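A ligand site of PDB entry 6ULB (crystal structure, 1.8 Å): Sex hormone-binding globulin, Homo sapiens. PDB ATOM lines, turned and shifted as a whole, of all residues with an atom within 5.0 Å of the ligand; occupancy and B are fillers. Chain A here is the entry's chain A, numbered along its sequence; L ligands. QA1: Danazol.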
ATOM      1  N   LEU A  34     -22.112   2.879 -27.720  1.00  0.00           N
ATOM      2  CA  LEU A  34     -23.137   3.378 -26.803  1.00  0.00           C
ATOM      3  C   LEU A  34     -24.226   2.336 -26.552  1.00  0.00           C
ATOM      4  O   LEU A  34     -24.862   2.367 -25.498  1.00  0.00           O
ATOM      5  CB  LEU A  34     -23.741   4.663 -27.351  1.00  0.00           C
ATOM      6  CG  LEU A  34     -22.970   5.902 -26.896  1.00  0.00           C
ATOM      7  CD1 LEU A  34     -23.728   7.143 -27.287  1.00  0.00           C
ATOM      8  CD2 LEU A  34     -22.701   5.853 -25.385  1.00  0.00           C
ATOM      9  N   THR A  40     -22.557   3.950 -16.362  1.00  0.00           N
ATOM     10  CA  THR A  40     -22.455   5.310 -16.890  1.00  0.00           C
ATOM     11  C   THR A  40     -21.817   6.214 -15.848  1.00  0.00           C
ATOM     12  O   THR A  40     -22.386   7.242 -15.466  1.00  0.00           O
ATOM     13  CB  THR A  40     -23.836   5.831 -17.302  1.00  0.00           C
ATOM     14  OG1 THR A  40     -24.743   5.760 -16.192  1.00  0.00           O
ATOM     15  CG2 THR A  40     -24.394   4.987 -18.435  1.00  0.00           C
ATOM     16  N   SER A  41     -20.648   5.822 -15.349  1.00  0.00           N
ATOM     17  CA  SER A  41     -19.879   6.641 -14.432  1.00  0.00           C
ATOM     18  C   SER A  41     -18.390   6.466 -14.729  1.00  0.00           C
ATOM     19  O   SER A  41     -17.967   5.458 -15.313  1.00  0.00           O
ATOM     20  CB  SER A  41     -20.178   6.295 -12.963  1.00  0.00           C
ATOM     21  OG  SER A  41     -19.908   4.925 -12.695  1.00  0.00           O
ATOM     22  N   SER A  42     -17.621   7.457 -14.312  1.00  0.00           N
ATOM     23  CA  SER A  42     -16.175   7.485 -14.455  1.00  0.00           C
ATOM     24  C   SER A  42     -15.599   8.093 -13.192  1.00  0.00           C
ATOM     25  O   SER A  42     -16.215   8.964 -12.566  1.00  0.00           O
ATOM     26  CB  SER A  42     -15.724   8.322 -15.677  1.00  0.00           C
ATOM     27  OG  SER A  42     -16.184   7.763 -16.905  1.00  0.00           O
ATOM     28  N   PHE A  56     -11.141  16.401 -19.107  1.00  0.00           N
ATOM     29  CA  PHE A  56     -11.508  15.483 -20.184  1.00  0.00           C
ATOM     30  C   PHE A  56     -12.634  16.078 -21.014  1.00  0.00           C
ATOM     31  O   PHE A  56     -13.334  16.992 -20.588  1.00  0.00           O
ATOM     32  CB  PHE A  56     -11.864  14.072 -19.649  1.00  0.00           C
ATOM     33  CG  PHE A  56     -13.220  13.952 -18.985  1.00  0.00           C
ATOM     34  CD1 PHE A  56     -14.363  13.670 -19.744  1.00  0.00           C
ATOM     35  CD2 PHE A  56     -13.348  14.034 -17.604  1.00  0.00           C
ATOM     36  CE1 PHE A  56     -15.601  13.512 -19.125  1.00  0.00           C
ATOM     37  CE2 PHE A  56     -14.589  13.865 -16.977  1.00  0.00           C
ATOM     38  CZ  PHE A  56     -15.727  13.606 -17.752  1.00  0.00           C
ATOM     39  N   GLY A  58     -15.756  14.789 -24.047  1.00  0.00           N
ATOM     40  CA  GLY A  58     -16.421  13.656 -24.672  1.00  0.00           C
ATOM     41  C   GLY A  58     -17.441  14.116 -25.687  1.00  0.00           C
ATOM     42  O   GLY A  58     -17.988  15.215 -25.582  1.00  0.00           O
ATOM     43  N   ASP A  59     -17.714  13.264 -26.658  1.00  0.00           N
ATOM     44  CA  ASP A  59     -18.726  13.622 -27.669  1.00  0.00           C
ATOM     45  C   ASP A  59     -19.285  12.396 -28.375  1.00  0.00           C
ATOM     46  O   ASP A  59     -18.799  11.301 -28.179  1.00  0.00           O
ATOM     47  CB  ASP A  59     -18.173  14.611 -28.702  1.00  0.00           C
ATOM     48  CG  ASP A  59     -17.164  14.077 -29.706  1.00  0.00           C
ATOM     49  OD1 ASP A  59     -17.100  12.891 -29.881  1.00  0.00           O
ATOM     50  OD2 ASP A  59     -16.460  14.858 -30.285  1.00  0.00           O
ATOM     51  N   THR A  60     -20.372  12.635 -29.081  1.00  0.00           N
ATOM     52  CA  THR A  60     -20.842  11.717 -30.126  1.00  0.00           C
ATOM     53  C   THR A  60     -20.733  12.525 -31.427  1.00  0.00           C
ATOM     54  O   THR A  60     -20.741  11.917 -32.461  1.00  0.00           O
ATOM     55  CB  THR A  60     -22.243  11.136 -29.957  1.00  0.00           C
ATOM     56  OG1 THR A  60     -23.162  12.114 -30.384  1.00  0.00           O
ATOM     57  CG2 THR A  60     -22.555  10.585 -28.595  1.00  0.00           C
ATOM     58  N   ASP A  65     -22.986  17.672 -29.989  1.00  0.00           N
ATOM     59  CA  ASP A  65     -23.276  16.697 -28.925  1.00  0.00           C
ATOM     60  C   ASP A  65     -21.953  16.414 -28.208  1.00  0.00           C
ATOM     61  O   ASP A  65     -21.265  15.428 -28.460  1.00  0.00           O
ATOM     62  CB  ASP A  65     -23.923  15.437 -29.515  1.00  0.00           C
ATOM     63  CG  ASP A  65     -24.530  14.520 -28.442  1.00  0.00           C
ATOM     64  OD1 ASP A  65     -25.187  15.026 -27.495  1.00  0.00           O
ATOM     65  OD2 ASP A  65     -24.326  13.293 -28.529  1.00  0.00           O
ATOM     66  N   TRP A  66     -21.589  17.311 -27.295  1.00  0.00           N
ATOM     67  CA  TRP A  66     -20.273  17.249 -26.676  1.00  0.00           C
ATOM     68  C   TRP A  66     -20.326  17.771 -25.241  1.00  0.00           C
ATOM     69  O   TRP A  66     -21.293  18.391 -24.815  1.00  0.00           O
ATOM     70  CB  TRP A  66     -19.222  18.016 -27.503  1.00  0.00           C
ATOM     71  CG  TRP A  66     -19.514  19.498 -27.660  1.00  0.00           C
ATOM     72  CD1 TRP A  66     -20.144  20.090 -28.710  1.00  0.00           C
ATOM     73  CD2 TRP A  66     -19.134  20.549 -26.756  1.00  0.00           C
ATOM     74  NE1 TRP A  66     -20.206  21.473 -28.497  1.00  0.00           N
ATOM     75  CE2 TRP A  66     -19.590  21.761 -27.314  1.00  0.00           C
ATOM     76  CE3 TRP A  66     -18.462  20.578 -25.532  1.00  0.00           C
ATOM     77  CZ2 TRP A  66     -19.397  22.996 -26.677  1.00  0.00           C
ATOM     78  CZ3 TRP A  66     -18.269  21.812 -24.895  1.00  0.00           C
ATOM     79  CH2 TRP A  66     -18.728  22.999 -25.480  1.00  0.00           C
ATOM     80  N   PHE A  67     -19.237  17.497 -24.510  1.00  0.00           N
ATOM     81  CA  PHE A  67     -19.137  17.742 -23.081  1.00  0.00           C
ATOM     82  C   PHE A  67     -17.676  18.001 -22.749  1.00  0.00           C
ATOM     83  O   PHE A  67     -16.784  17.372 -23.306  1.00  0.00           O
ATOM     84  CB  PHE A  67     -19.687  16.526 -22.313  1.00  0.00           C
ATOM     85  CG  PHE A  67     -19.520  16.576 -20.804  1.00  0.00           C
ATOM     86  CD1 PHE A  67     -18.311  16.267 -20.192  1.00  0.00           C
ATOM     87  CD2 PHE A  67     -20.623  16.855 -19.986  1.00  0.00           C
ATOM     88  CE1 PHE A  67     -18.177  16.283 -18.785  1.00  0.00           C
ATOM     89  CE2 PHE A  67     -20.507  16.862 -18.586  1.00  0.00           C
ATOM     90  CZ  PHE A  67     -19.284  16.566 -17.988  1.00  0.00           C
ATOM     91  N   LEU A  80     -21.359  21.993 -21.794  1.00  0.00           N
ATOM     92  CA  LEU A  80     -22.126  20.887 -22.360  1.00  0.00           C
ATOM     93  C   LEU A  80     -22.985  21.454 -23.486  1.00  0.00           C
ATOM     94  O   LEU A  80     -23.536  22.540 -23.364  1.00  0.00           O
ATOM     95  CB  LEU A  80     -22.977  20.240 -21.258  1.00  0.00           C
ATOM     96  CG  LEU A  80     -24.015  19.128 -21.451  1.00  0.00           C
ATOM     97  CD1 LEU A  80     -24.304  18.497 -20.098  1.00  0.00           C
ATOM     98  CD2 LEU A  80     -25.275  19.697 -22.052  1.00  0.00           C
ATOM     99  N   ASN A  82     -25.807  19.693 -26.155  1.00  0.00           N
ATOM    100  CA  ASN A  82     -26.506  18.595 -26.805  1.00  0.00           C
ATOM    101  C   ASN A  82     -27.933  19.033 -27.109  1.00  0.00           C
ATOM    102  O   ASN A  82     -28.277  20.213 -27.011  1.00  0.00           O
ATOM    103  CB  ASN A  82     -26.409  17.323 -25.933  1.00  0.00           C
ATOM    104  CG  ASN A  82     -27.242  17.405 -24.642  1.00  0.00           C
ATOM    105  OD1 ASN A  82     -28.140  18.226 -24.529  1.00  0.00           O
ATOM    106  ND2 ASN A  82     -26.946  16.521 -23.677  1.00  0.00           N
ATOM    107  N   TRP A  84     -30.685  18.613 -25.626  1.00  0.00           N
ATOM    108  CA  TRP A  84     -31.522  19.031 -24.506  1.00  0.00           C
ATOM    109  C   TRP A  84     -30.980  20.226 -23.748  1.00  0.00           C
ATOM    110  O   TRP A  84     -31.763  20.940 -23.130  1.00  0.00           O
ATOM    111  CB  TRP A  84     -31.699  17.870 -23.517  1.00  0.00           C
ATOM    112  CG  TRP A  84     -32.353  16.688 -24.148  1.00  0.00           C
ATOM    113  CD1 TRP A  84     -33.688  16.500 -24.342  1.00  0.00           C
ATOM    114  CD2 TRP A  84     -31.696  15.539 -24.686  1.00  0.00           C
ATOM    115  NE1 TRP A  84     -33.904  15.284 -24.972  1.00  0.00           N
ATOM    116  CE2 TRP A  84     -32.699  14.676 -25.183  1.00  0.00           C
ATOM    117  CE3 TRP A  84     -30.365  15.139 -24.787  1.00  0.00           C
ATOM    118  CZ2 TRP A  84     -32.402  13.453 -25.783  1.00  0.00           C
ATOM    119  CZ3 TRP A  84     -30.070  13.924 -25.376  1.00  0.00           C
ATOM    120  CH2 TRP A  84     -31.085  13.100 -25.869  1.00  0.00           C
ATOM    121  N   VAL A 105     -17.713  11.345 -12.042  1.00  0.00           N
ATOM    122  CA  VAL A 105     -18.798  11.852 -12.877  1.00  0.00           C
ATOM    123  C   VAL A 105     -19.792  10.733 -13.079  1.00  0.00           C
ATOM    124  O   VAL A 105     -19.401   9.600 -13.430  1.00  0.00           O
ATOM    125  CB  VAL A 105     -18.269  12.360 -14.233  1.00  0.00           C
ATOM    126  CG1 VAL A 105     -19.438  12.808 -15.105  1.00  0.00           C
ATOM    127  CG2 VAL A 105     -17.257  13.488 -14.023  1.00  0.00           C
ATOM    128  N   LYS A 106     -21.064  11.007 -12.835  1.00  0.00           N
ATOM    129  CA  LYS A 106     -22.084   9.966 -12.914  1.00  0.00           C
ATOM    130  C   LYS A 106     -23.262  10.463 -13.715  1.00  0.00           C
ATOM    131  O   LYS A 106     -23.747  11.576 -13.503  1.00  0.00           O
ATOM    132  CB  LYS A 106     -22.577   9.537 -11.531  1.00  0.00           C
ATOM    133  CG  LYS A 106     -21.500   9.038 -10.570  1.00  0.00           C
ATOM    134  CD  LYS A 106     -22.060   8.865  -9.159  1.00  0.00           C
ATOM    135  CE  LYS A 106     -21.062   8.195  -8.222  1.00  0.00           C
ATOM    136  NZ  LYS A 106     -21.587   8.075  -6.822  1.00  0.00           N
ATOM    137  N   MET A 107     -23.753   9.632 -14.622  1.00  0.00           N
ATOM    138  CA  MET A 107     -25.002   9.902 -15.308  1.00  0.00           C
ATOM    139  C   MET A 107     -26.089   9.081 -14.642  1.00  0.00           C
ATOM    140  O   MET A 107     -26.012   7.839 -14.622  1.00  0.00           O
ATOM    141  CB  MET A 107     -24.888   9.574 -16.794  1.00  0.00           C
ATOM    142  CG  MET A 107     -25.992  10.171 -17.628  1.00  0.00           C
ATOM    143  SD  MET A 107     -25.649   9.990 -19.376  1.00  0.00           S
ATOM    144  CE  MET A 107     -23.989   9.296 -19.304  1.00  0.00           C
ATOM    145  N   VAL A 112     -26.567  14.683 -14.909  1.00  0.00           N
ATOM    146  CA  VAL A 112     -25.139  14.436 -14.770  1.00  0.00           C
ATOM    147  C   VAL A 112     -24.701  14.979 -13.402  1.00  0.00           C
ATOM    148  O   VAL A 112     -24.991  16.129 -13.070  1.00  0.00           O
ATOM    149  CB  VAL A 112     -24.340  15.098 -15.907  1.00  0.00           C
ATOM    150  CG1 VAL A 112     -22.852  15.080 -15.609  1.00  0.00           C
ATOM    151  CG2 VAL A 112     -24.693  14.426 -17.219  1.00  0.00           C
ATOM    152  N   SER A 128     -29.936  15.062 -20.317  1.00  0.00           N
ATOM    153  CA  SER A 128     -29.661  13.995 -21.277  1.00  0.00           C
ATOM    154  C   SER A 128     -30.814  13.008 -21.290  1.00  0.00           C
ATOM    155  O   SER A 128     -31.419  12.728 -20.254  1.00  0.00           O
ATOM    156  CB  SER A 128     -28.352  13.262 -20.948  1.00  0.00           C
ATOM    157  OG  SER A 128     -28.011  12.332 -21.978  1.00  0.00           O
ATOM    158  N   LEU A 131     -28.590   7.288 -22.943  1.00  0.00           N
ATOM    159  CA  LEU A 131     -27.408   7.105 -23.772  1.00  0.00           C
ATOM    160  C   LEU A 131     -27.667   6.083 -24.867  1.00  0.00           C
ATOM    161  O   LEU A 131     -27.444   6.346 -26.057  1.00  0.00           O
ATOM    162  CB  LEU A 131     -26.215   6.670 -22.911  1.00  0.00           C
ATOM    163  CG  LEU A 131     -25.486   7.729 -22.089  1.00  0.00           C
ATOM    164  CD1 LEU A 131     -24.038   7.344 -21.853  1.00  0.00           C
ATOM    165  CD2 LEU A 131     -25.583   9.081 -22.786  1.00  0.00           C
ATOM    166  N   MET A 139     -19.420   6.972 -28.828  1.00  0.00           N
ATOM    167  CA  MET A 139     -18.996   8.072 -27.964  1.00  0.00           C
ATOM    168  C   MET A 139     -17.479   8.058 -27.795  1.00  0.00           C
ATOM    169  O   MET A 139     -16.878   6.998 -27.599  1.00  0.00           O
ATOM    170  CB  MET A 139     -19.678   7.994 -26.594  1.00  0.00           C
ATOM    171  CG  MET A 139     -19.230   9.099 -25.637  1.00  0.00           C
ATOM    172  SD  MET A 139     -19.980   8.942 -24.016  1.00  0.00           S
ATOM    173  CE  MET A 139     -21.656   9.339 -24.426  1.00  0.00           C
ATOM    174  N   ILE A 141     -14.143   9.657 -25.648  1.00  0.00           N
ATOM    175  CA  ILE A 141     -13.646  10.357 -24.466  1.00  0.00           C
ATOM    176  C   ILE A 141     -12.172  10.675 -24.683  1.00  0.00           C
ATOM    177  O   ILE A 141     -11.385   9.783 -24.983  1.00  0.00           O
ATOM    178  CB  ILE A 141     -13.855   9.518 -23.180  1.00  0.00           C
ATOM    179  CG1 ILE A 141     -15.346   9.331 -22.901  1.00  0.00           C
ATOM    180  CG2 ILE A 141     -13.202  10.214 -21.994  1.00  0.00           C
ATOM    181  CD1 ILE A 141     -15.604   8.498 -21.661  1.00  0.00           C
ATOM    182  N   LEU A 171     -16.166   4.821 -17.782  1.00  0.00           N
ATOM    183  CA  LEU A 171     -17.395   4.151 -18.216  1.00  0.00           C
ATOM    184  C   LEU A 171     -17.195   2.640 -18.135  1.00  0.00           C
ATOM    185  O   LEU A 171     -16.770   2.122 -17.092  1.00  0.00           O
ATOM    186  CB  LEU A 171     -17.788   4.680 -19.599  1.00  0.00           C
ATOM    187  CG  LEU A 171     -18.129   6.160 -19.698  1.00  0.00           C
ATOM    188  CD1 LEU A 171     -18.304   6.568 -21.153  1.00  0.00           C
ATOM    189  CD2 LEU A 171     -19.392   6.468 -18.902  1.00  0.00           C
HETATM  190  CAD QA1 L   1     -21.820  13.078 -23.538  1.00  0.00           C
HETATM  191  CAE QA1 L   1     -23.247  13.531 -23.190  1.00  0.00           C
HETATM  192  CAF QA1 L   1     -20.897  13.146 -22.313  1.00  0.00           C
HETATM  193  CAG QA1 L   1     -21.482  12.145 -21.281  1.00  0.00           C
HETATM  194  CAH QA1 L   1     -20.562  12.000 -20.056  1.00  0.00           C
HETATM  195  CAI QA1 L   1     -23.865  12.602 -22.112  1.00  0.00           C
HETATM  196  CAJ QA1 L   1     -23.884  13.426 -24.600  1.00  0.00           C
HETATM  197  CAK QA1 L   1     -22.940  12.555 -20.866  1.00  0.00           C
HETATM  198  CAL QA1 L   1     -21.458  13.924 -24.775  1.00  0.00           C
HETATM  199  CAM QA1 L   1     -19.543  12.718 -22.763  1.00  0.00           C
HETATM  200  CAN QA1 L   1     -22.821  14.096 -25.504  1.00  0.00           C
HETATM  201  CAO QA1 L   1     -19.245  11.765 -20.513  1.00  0.00           C
HETATM  202  CAP QA1 L   1     -23.271  14.985 -22.685  1.00  0.00           C
HETATM  203  CAQ QA1 L   1     -18.645  12.467 -21.576  1.00  0.00           C
HETATM  204  CAR QA1 L   1     -21.103  10.817 -19.247  1.00  0.00           C
HETATM  205  CAS QA1 L   1     -20.568  13.203 -19.114  1.00  0.00           C
HETATM  206  CAT QA1 L   1     -24.040  11.992 -25.029  1.00  0.00           C
HETATM  207  CAU QA1 L   1     -18.413  10.880 -19.829  1.00  0.00           C
HETATM  208  CAV QA1 L   1     -20.136  10.275 -18.403  1.00  0.00           C
HETATM  209  CAW QA1 L   1     -18.842  10.281 -18.735  1.00  0.00           C
HETATM  210  CAX QA1 L   1     -20.293   9.633 -17.244  1.00  0.00           C
HETATM  211  CAY QA1 L   1     -24.198  10.897 -25.362  1.00  0.00           C
HETATM  212  NAC QA1 L   1     -19.100   9.240 -16.791  1.00  0.00           N
HETATM  213  OAA QA1 L   1     -25.163  14.071 -24.723  1.00  0.00           O
HETATM  214  OAB QA1 L   1     -18.124   9.666 -17.769  1.00  0.00           O
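O of Val 105 sits close to NAC of the ligand, 3.4 Å away. Thr 40 touches the ligand. Ser 41 touches the ligand. Phe 56 touches the ligand. CA of Gly 58 touches CAM of the ligand, at 3.8 Å. Asp 59 touches the ligand. Thr 60 touches the ligand. Trp 66 touches the ligand (N to CAN, 3.9 Å). Phe 67 touches the ligand (CB to CAF, 3.6 Å). Met 107 touches the ligand. Leu 131 touches the ligand (CD2 to CAY, 3.4 Å). Met 139 touches the ligand. Leu 171 touches the ligand (CD2 to NAC, 3.5 Å). Hydrophobic or aromatic side chains within 4 Å of the ligand: Phe 56, Phe 67, Val 105, Met 107, Leu 131, Met 139 and Leu 171. The nearest printed residue that does not touch the ligand is Ile 141 (4.1 Å).
An oxygen (OAB) of the ligand sits at hydrogen-bond distance from the side-chain hydroxyl (OG) of Ser 42 (2.9 Å). NAC of the ligand lies within hydrogen-bond range of N of Ser 42 (3.4 Å). The side-chain amide nitrogen (ND2) of Asn 82 sits at hydrogen-bond distance from an oxygen (OAA) of the ligand (3.2 Å). OD1 of Asp 65 is in hydrogen-bond range of OAA of the ligand.
OD2 of Asp 65 is in hydrogen-bond range of OG1 of Thr 60, at 2.5 Å. The backbone NH of Val 105 lies within hydrogen-bond range of the backbone carbonyl oxygen of Ser 42 (2.9 Å). N of Phe 67 is in hydrogen-bond range of O of Gly 58 (2.8 Å). The side-chain amide oxygen (OD1) of Asn 82 lies within hydrogen-bond range of the backbone NH (N) of Trp 84 (2.8 Å). The backbone carbonyl oxygen (O) of Ser 41 lies within hydrogen-bond range of the backbone NH (N) of Leu 171, at 3.1 Å. The backbone carbonyl oxygen of Thr 40 sits at hydrogen-bond distance from the backbone NH of Met 107, 2.9 Å away. OG of Ser 42 is in hydrogen-bond range of N of Leu 171 (3.1 Å).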
